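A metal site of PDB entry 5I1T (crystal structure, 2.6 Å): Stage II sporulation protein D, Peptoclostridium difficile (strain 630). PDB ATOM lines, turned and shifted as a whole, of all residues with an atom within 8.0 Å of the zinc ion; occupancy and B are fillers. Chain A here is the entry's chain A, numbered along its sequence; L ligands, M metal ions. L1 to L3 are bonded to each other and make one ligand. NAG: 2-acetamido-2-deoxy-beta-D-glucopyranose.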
ATOM      1  N   TYR A  54      22.819  -7.819  10.781  1.00  0.00           N
ATOM      2  CA  TYR A  54      24.079  -8.441  11.103  1.00  0.00           C
ATOM      3  C   TYR A  54      25.184  -7.697  10.370  1.00  0.00           C
ATOM      4  O   TYR A  54      25.198  -7.628   9.142  1.00  0.00           O
ATOM      5  CB  TYR A  54      24.082  -9.941  10.748  1.00  0.00           C
ATOM      6  CG  TYR A  54      25.431 -10.602  11.022  1.00  0.00           C
ATOM      7  CD1 TYR A  54      25.856 -10.846  12.330  1.00  0.00           C
ATOM      8  CD2 TYR A  54      26.268 -11.000   9.969  1.00  0.00           C
ATOM      9  CE1 TYR A  54      27.086 -11.434  12.578  1.00  0.00           C
ATOM     10  CE2 TYR A  54      27.491 -11.605  10.201  1.00  0.00           C
ATOM     11  CZ  TYR A  54      27.899 -11.818  11.520  1.00  0.00           C
ATOM     12  OH  TYR A  54      29.127 -12.400  11.755  1.00  0.00           O
ATOM     13  N   HIS A  56      28.581  -7.927   9.213  1.00  0.00           N
ATOM     14  CA  HIS A  56      29.558  -8.994   8.953  1.00  0.00           C
ATOM     15  C   HIS A  56      30.998  -8.642   9.268  1.00  0.00           C
ATOM     16  O   HIS A  56      31.796  -9.516   9.465  1.00  0.00           O
ATOM     17  CB  HIS A  56      29.445  -9.509   7.506  1.00  0.00           C
ATOM     18  CG  HIS A  56      30.110  -8.625   6.484  1.00  0.00           C
ATOM     19  ND1 HIS A  56      29.600  -7.405   6.092  1.00  0.00           N
ATOM     20  CD2 HIS A  56      31.222  -8.821   5.733  1.00  0.00           C
ATOM     21  CE1 HIS A  56      30.375  -6.874   5.164  1.00  0.00           C
ATOM     22  NE2 HIS A  56      31.366  -7.719   4.918  1.00  0.00           N
ATOM     23  N   TYR A  69      19.049   2.638   7.522  1.00  0.00           N
ATOM     24  CA  TYR A  69      19.691   1.462   6.960  1.00  0.00           C
ATOM     25  C   TYR A  69      19.709   1.514   5.412  1.00  0.00           C
ATOM     26  O   TYR A  69      20.723   1.218   4.784  1.00  0.00           O
ATOM     27  CB  TYR A  69      18.994   0.169   7.471  1.00  0.00           C
ATOM     28  CG  TYR A  69      19.343  -1.063   6.643  1.00  0.00           C
ATOM     29  CD1 TYR A  69      20.591  -1.667   6.729  1.00  0.00           C
ATOM     30  CD2 TYR A  69      18.413  -1.593   5.752  1.00  0.00           C
ATOM     31  CE1 TYR A  69      20.904  -2.774   5.945  1.00  0.00           C
ATOM     32  CE2 TYR A  69      18.712  -2.684   4.962  1.00  0.00           C
ATOM     33  CZ  TYR A  69      19.958  -3.275   5.054  1.00  0.00           C
ATOM     34  OH  TYR A  69      20.221  -4.347   4.247  1.00  0.00           O
ATOM     35  N   TYR A  97      13.535  -6.007   0.026  1.00  0.00           N
ATOM     36  CA  TYR A  97      14.414  -7.138   0.370  1.00  0.00           C
ATOM     37  C   TYR A  97      14.284  -7.439   1.856  1.00  0.00           C
ATOM     38  O   TYR A  97      14.093  -8.580   2.252  1.00  0.00           O
ATOM     39  CB  TYR A  97      15.868  -6.817   0.013  1.00  0.00           C
ATOM     40  CG  TYR A  97      16.787  -8.013  -0.072  1.00  0.00           C
ATOM     41  CD1 TYR A  97      17.405  -8.517   1.063  1.00  0.00           C
ATOM     42  CD2 TYR A  97      17.041  -8.630  -1.295  1.00  0.00           C
ATOM     43  CE1 TYR A  97      18.253  -9.618   0.988  1.00  0.00           C
ATOM     44  CE2 TYR A  97      17.880  -9.740  -1.389  1.00  0.00           C
ATOM     45  CZ  TYR A  97      18.494 -10.222  -0.251  1.00  0.00           C
ATOM     46  OH  TYR A  97      19.349 -11.312  -0.330  1.00  0.00           O
ATOM     47  N   LYS A 101      12.462 -10.776   3.615  1.00  0.00           N
ATOM     48  CA  LYS A 101      13.169 -11.627   4.578  1.00  0.00           C
ATOM     49  C   LYS A 101      12.441 -11.737   5.911  1.00  0.00           C
ATOM     50  O   LYS A 101      12.423 -12.799   6.497  1.00  0.00           O
ATOM     51  CB  LYS A 101      14.600 -11.153   4.812  1.00  0.00           C
ATOM     52  CG  LYS A 101      15.526 -11.226   3.607  1.00  0.00           C
ATOM     53  CD  LYS A 101      15.898 -12.637   3.205  1.00  0.00           C
ATOM     54  CE  LYS A 101      16.901 -12.582   2.077  1.00  0.00           C
ATOM     55  NZ  LYS A 101      17.382 -13.934   1.681  1.00  0.00           N
ATOM     56  N   SER A 107      17.663 -16.903   8.261  1.00  0.00           N
ATOM     57  CA  SER A 107      18.840 -17.399   7.534  1.00  0.00           C
ATOM     58  C   SER A 107      19.731 -18.319   8.357  1.00  0.00           C
ATOM     59  O   SER A 107      19.733 -18.274   9.592  1.00  0.00           O
ATOM     60  CB  SER A 107      19.685 -16.223   7.023  1.00  0.00           C
ATOM     61  OG  SER A 107      20.809 -16.711   6.291  1.00  0.00           O
ATOM     62  N   LYS A 109      23.116 -18.381   7.892  1.00  0.00           N
ATOM     63  CA  LYS A 109      24.241 -17.482   8.160  1.00  0.00           C
ATOM     64  C   LYS A 109      24.086 -16.607   9.411  1.00  0.00           C
ATOM     65  O   LYS A 109      24.951 -16.585  10.272  1.00  0.00           O
ATOM     66  CB  LYS A 109      24.451 -16.553   6.961  1.00  0.00           C
ATOM     67  CG  LYS A 109      25.313 -17.078   5.833  1.00  0.00           C
ATOM     68  CD  LYS A 109      26.782 -16.862   6.140  1.00  0.00           C
ATOM     69  CE  LYS A 109      27.637 -17.085   4.917  1.00  0.00           C
ATOM     70  NZ  LYS A 109      29.070 -16.845   5.225  1.00  0.00           N
ATOM     71  N   HIS A 110      22.977 -15.863   9.464  1.00  0.00           N
ATOM     72  CA  HIS A 110      22.695 -14.945  10.571  1.00  0.00           C
ATOM     73  C   HIS A 110      21.242 -15.112  11.036  1.00  0.00           C
ATOM     74  O   HIS A 110      20.356 -14.395  10.581  1.00  0.00           O
ATOM     75  CB  HIS A 110      22.992 -13.493  10.133  1.00  0.00           C
ATOM     76  CG  HIS A 110      22.480 -13.137   8.765  1.00  0.00           C
ATOM     77  ND1 HIS A 110      21.159 -12.843   8.502  1.00  0.00           N
ATOM     78  CD2 HIS A 110      23.126 -12.998   7.578  1.00  0.00           C
ATOM     79  CE1 HIS A 110      21.013 -12.559   7.222  1.00  0.00           C
ATOM     80  NE2 HIS A 110      22.195 -12.629   6.644  1.00  0.00           N
ATOM     81  N   ALA A 113      19.345 -12.014  12.702  1.00  0.00           N
ATOM     82  CA  ALA A 113      19.213 -10.822  11.860  1.00  0.00           C
ATOM     83  C   ALA A 113      18.427 -11.085  10.563  1.00  0.00           C
ATOM     84  O   ALA A 113      18.542 -12.144   9.967  1.00  0.00           O
ATOM     85  CB  ALA A 113      20.601 -10.286  11.517  1.00  0.00           C
ATOM     86  N   VAL A 114      17.657 -10.095  10.141  1.00  0.00           N
ATOM     87  CA  VAL A 114      16.842 -10.211   8.923  1.00  0.00           C
ATOM     88  C   VAL A 114      17.725 -10.137   7.670  1.00  0.00           C
ATOM     89  O   VAL A 114      17.526 -10.888   6.715  1.00  0.00           O
ATOM     90  CB  VAL A 114      15.748  -9.125   8.890  1.00  0.00           C
ATOM     91  CG1 VAL A 114      14.926  -9.215   7.621  1.00  0.00           C
ATOM     92  CG2 VAL A 114      14.843  -9.293  10.098  1.00  0.00           C
ATOM     93  N   VAL A 115      18.672  -9.206   7.691  1.00  0.00           N
ATOM     94  CA  VAL A 115      19.623  -8.997   6.608  1.00  0.00           C
ATOM     95  C   VAL A 115      21.013  -8.751   7.196  1.00  0.00           C
ATOM     96  O   VAL A 115      21.142  -8.495   8.399  1.00  0.00           O
ATOM     97  CB  VAL A 115      19.246  -7.760   5.743  1.00  0.00           C
ATOM     98  CG1 VAL A 115      17.953  -8.009   4.981  1.00  0.00           C
ATOM     99  CG2 VAL A 115      19.139  -6.504   6.612  1.00  0.00           C
ATOM    100  N   CYS A 116      22.030  -8.859   6.351  1.00  0.00           N
ATOM    101  CA  CYS A 116      23.400  -8.589   6.794  1.00  0.00           C
ATOM    102  C   CYS A 116      24.031  -7.581   5.846  1.00  0.00           C
ATOM    103  O   CYS A 116      23.512  -7.338   4.766  1.00  0.00           O
ATOM    104  CB  CYS A 116      24.247  -9.852   6.885  1.00  0.00           C
ATOM    105  SG  CYS A 116      24.615 -10.672   5.320  1.00  0.00           S
ATOM    106  N   THR A 117      25.167  -7.038   6.269  1.00  0.00           N
ATOM    107  CA  THR A 117      25.888  -5.991   5.511  1.00  0.00           C
ATOM    108  C   THR A 117      26.839  -6.497   4.412  1.00  0.00           C
ATOM    109  O   THR A 117      27.647  -5.714   3.909  1.00  0.00           O
ATOM    110  CB  THR A 117      26.700  -5.086   6.480  1.00  0.00           C
ATOM    111  OG1 THR A 117      27.567  -5.903   7.271  1.00  0.00           O
ATOM    112  CG2 THR A 117      25.776  -4.309   7.400  1.00  0.00           C
ATOM    113  N   ASP A 118      26.708  -7.760   4.020  1.00  0.00           N
ATOM    114  CA  ASP A 118      27.566  -8.391   2.999  1.00  0.00           C
ATOM    115  C   ASP A 118      26.818  -8.552   1.661  1.00  0.00           C
ATOM    116  O   ASP A 118      25.841  -9.312   1.554  1.00  0.00           O
ATOM    117  CB  ASP A 118      28.069  -9.741   3.526  1.00  0.00           C
ATOM    118  CG  ASP A 118      29.101 -10.404   2.616  1.00  0.00           C
ATOM    119  OD1 ASP A 118      29.464  -9.836   1.557  1.00  0.00           O
ATOM    120  OD2 ASP A 118      29.555 -11.509   2.969  1.00  0.00           O
ATOM    121  N   TYR A 119      27.285  -7.846   0.625  1.00  0.00           N
ATOM    122  CA  TYR A 119      26.668  -7.898  -0.701  1.00  0.00           C
ATOM    123  C   TYR A 119      26.703  -9.306  -1.326  1.00  0.00           C
ATOM    124  O   TYR A 119      25.971  -9.574  -2.273  1.00  0.00           O
ATOM    125  CB  TYR A 119      27.336  -6.872  -1.653  1.00  0.00           C
ATOM    126  CG  TYR A 119      28.727  -7.238  -2.163  1.00  0.00           C
ATOM    127  CD1 TYR A 119      29.869  -6.957  -1.426  1.00  0.00           C
ATOM    128  CD2 TYR A 119      28.888  -7.853  -3.411  1.00  0.00           C
ATOM    129  CE1 TYR A 119      31.124  -7.299  -1.896  1.00  0.00           C
ATOM    130  CE2 TYR A 119      30.152  -8.195  -3.890  1.00  0.00           C
ATOM    131  CZ  TYR A 119      31.264  -7.911  -3.124  1.00  0.00           C
ATOM    132  OH  TYR A 119      32.516  -8.237  -3.578  1.00  0.00           O
ATOM    133  N   LYS A 120      27.553 -10.178  -0.791  1.00  0.00           N
ATOM    134  CA  LYS A 120      27.663 -11.576  -1.270  1.00  0.00           C
ATOM    135  C   LYS A 120      26.543 -12.465  -0.712  1.00  0.00           C
ATOM    136  O   LYS A 120      26.325 -13.578  -1.207  1.00  0.00           O
ATOM    137  CB  LYS A 120      29.022 -12.174  -0.910  1.00  0.00           C
ATOM    138  CG  LYS A 120      30.189 -11.473  -1.585  1.00  0.00           C
ATOM    139  CD  LYS A 120      31.520 -11.909  -1.004  1.00  0.00           C
ATOM    140  CE  LYS A 120      32.642 -11.080  -1.585  1.00  0.00           C
ATOM    141  NZ  LYS A 120      33.929 -11.388  -0.910  1.00  0.00           N
ATOM    142  N   HIS A 121      25.861 -11.982   0.330  1.00  0.00           N
ATOM    143  CA  HIS A 121      24.776 -12.745   0.923  1.00  0.00           C
ATOM    144  C   HIS A 121      23.413 -12.039   0.801  1.00  0.00           C
ATOM    145  O   HIS A 121      22.447 -12.668   0.328  1.00  0.00           O
ATOM    146  CB  HIS A 121      25.064 -13.089   2.384  1.00  0.00           C
ATOM    147  CG  HIS A 121      24.098 -14.075   2.936  1.00  0.00           C
ATOM    148  ND1 HIS A 121      23.002 -13.714   3.687  1.00  0.00           N
ATOM    149  CD2 HIS A 121      24.010 -15.411   2.756  1.00  0.00           C
ATOM    150  CE1 HIS A 121      22.315 -14.801   3.997  1.00  0.00           C
ATOM    151  NE2 HIS A 121      22.898 -15.841   3.432  1.00  0.00           N
ATOM    152  N   CYS A 122      23.348 -10.763   1.236  1.00  0.00           N
ATOM    153  CA  CYS A 122      22.098  -9.958   1.139  1.00  0.00           C
ATOM    154  C   CYS A 122      22.321  -8.763   0.224  1.00  0.00           C
ATOM    155  O   CYS A 122      22.052  -8.849  -0.985  1.00  0.00           O
ATOM    156  CB  CYS A 122      21.559  -9.515   2.524  1.00  0.00           C
ATOM    157  SG  CYS A 122      20.885 -10.831   3.578  1.00  0.00           S
ATOM    158  N   GLN A 123      22.787  -7.648   0.790  1.00  0.00           N
ATOM    159  CA  GLN A 123      23.054  -6.445   0.000  1.00  0.00           C
ATOM    160  C   GLN A 123      24.093  -5.597   0.700  1.00  0.00           C
ATOM    161  O   GLN A 123      24.376  -5.773   1.888  1.00  0.00           O
ATOM    162  CB  GLN A 123      21.772  -5.673  -0.308  1.00  0.00           C
ATOM    163  CG  GLN A 123      20.854  -5.401   0.876  1.00  0.00           C
ATOM    164  CD  GLN A 123      19.492  -4.845   0.456  1.00  0.00           C
ATOM    165  OE1 GLN A 123      19.211  -4.679  -0.728  1.00  0.00           O
ATOM    166  NE2 GLN A 123      18.645  -4.555   1.448  1.00  0.00           N
HETATM  167  C1  NAG L   1      23.475 -10.903  -3.678  1.00  0.00           C
HETATM  168  C2  NAG L   1      21.987 -11.151  -3.870  1.00  0.00           C
HETATM  169  C3  NAG L   1      21.584 -12.326  -2.999  1.00  0.00           C
HETATM  170  C4  NAG L   1      22.428 -13.555  -3.369  1.00  0.00           C
HETATM  171  C5  NAG L   1      23.929 -13.205  -3.367  1.00  0.00           C
HETATM  172  C6  NAG L   1      24.803 -14.354  -3.877  1.00  0.00           C
HETATM  173  C7  NAG L   1      20.378  -9.362  -4.362  1.00  0.00           C
HETATM  174  C8  NAG L   1      19.801  -8.074  -3.865  1.00  0.00           C
HETATM  175  N2  NAG L   1      21.240  -9.952  -3.529  1.00  0.00           N
HETATM  176  O1  NAG L   1      23.877  -9.744  -4.398  1.00  0.00           O
HETATM  177  O3  NAG L   1      20.189 -12.582  -3.185  1.00  0.00           O
HETATM  178  O4  NAG L   1      22.192 -14.643  -2.446  1.00  0.00           O
HETATM  179  O5  NAG L   1      24.176 -12.049  -4.154  1.00  0.00           O
HETATM  180  O6  NAG L   1      24.409 -14.731  -5.198  1.00  0.00           O
HETATM  181  O7  NAG L   1      20.088  -9.810  -5.479  1.00  0.00           O
HETATM  182  C1  NAG L   2      21.693 -15.807  -3.103  1.00  0.00           C
HETATM  183  C2  NAG L   2      21.886 -17.038  -2.225  1.00  0.00           C
HETATM  184  C3  NAG L   2      21.131 -18.238  -2.784  1.00  0.00           C
HETATM  185  C4  NAG L   2      19.693 -17.884  -3.112  1.00  0.00           C
HETATM  186  C5  NAG L   2      19.598 -16.623  -3.964  1.00  0.00           C
HETATM  187  C6  NAG L   2      18.168 -16.140  -4.133  1.00  0.00           C
HETATM  188  C7  NAG L   2      23.996 -17.376  -0.988  1.00  0.00           C
HETATM  189  C8  NAG L   2      25.457 -17.718  -1.104  1.00  0.00           C
HETATM  190  N2  NAG L   2      23.309 -17.362  -2.128  1.00  0.00           N
HETATM  191  O3  NAG L   2      21.135 -19.295  -1.832  1.00  0.00           O
HETATM  192  O4  NAG L   2      19.110 -18.997  -3.819  1.00  0.00           O
HETATM  193  O5  NAG L   2      20.312 -15.565  -3.351  1.00  0.00           O
HETATM  194  O6  NAG L   2      17.622 -15.777  -2.860  1.00  0.00           O
HETATM  195  O7  NAG L   2      23.497 -17.116   0.099  1.00  0.00           O
HETATM  196  C1  NAG L   3      18.263 -19.832  -3.017  1.00  0.00           C
HETATM  197  C2  NAG L   3      17.120 -20.370  -3.882  1.00  0.00           C
HETATM  198  C3  NAG L   3      16.225 -21.316  -3.089  1.00  0.00           C
HETATM  199  C4  NAG L   3      17.060 -22.371  -2.350  1.00  0.00           C
HETATM  200  C5  NAG L   3      18.239 -21.734  -1.599  1.00  0.00           C
HETATM  201  C6  NAG L   3      19.148 -22.766  -0.939  1.00  0.00           C
HETATM  202  C7  NAG L   3      15.961 -19.108  -5.620  1.00  0.00           C
HETATM  203  C8  NAG L   3      15.292 -17.816  -5.977  1.00  0.00           C
HETATM  204  N2  NAG L   3      16.349 -19.237  -4.360  1.00  0.00           N
HETATM  205  O3  NAG L   3      15.289 -21.958  -3.956  1.00  0.00           O
HETATM  206  O4  NAG L   3      16.193 -23.045  -1.432  1.00  0.00           O
HETATM  207  O5  NAG L   3      19.007 -20.927  -2.500  1.00  0.00           O
HETATM  208  O6  NAG L   3      20.312 -22.976  -1.736  1.00  0.00           O
HETATM  209  O7  NAG L   3      16.144 -19.957  -6.479  1.00  0.00           O
HETATM  210 ZN    ZN M   1      22.691 -11.824   4.665  1.00  0.00          ZN
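Four residues have an atom within 4 Å of the zinc ion: His 110, Cys 116, His 121 and Cys 122. The nearest printed residue that does not touch the zinc ion is Val 115 (4.3 Å).
A nitrogen (N2) of NAG L1 lies within hydrogen-bond range of the backbone carbonyl oxygen of Cys 122 (2.9 Å). An oxygen (O3) of NAG L1 lies within hydrogen-bond range of the side-chain hydroxyl (OH) of Tyr 97, at 3.2 Å. An oxygen (O1) of NAG L1 sits at hydrogen-bond distance from the backbone carbonyl oxygen of Tyr 119, 3.0 Å away.
The side-chain hydroxyl (OH) of Tyr 97 sits at hydrogen-bond distance from the backbone carbonyl oxygen (O) of His 121 (3.4 Å). The backbone carbonyl oxygen of Ala 113 is in hydrogen-bond range of a ring nitrogen (ND1) of His 110, 3.1 Å away.
The zinc ion is bound by a ring nitrogen (ND1) of His 121, a ring nitrogen (NE2) of His 110, the side-chain sulfur of Cys 122 and the side-chain sulfur of Cys 116. The zinc ion has four donor atoms within binding distance.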
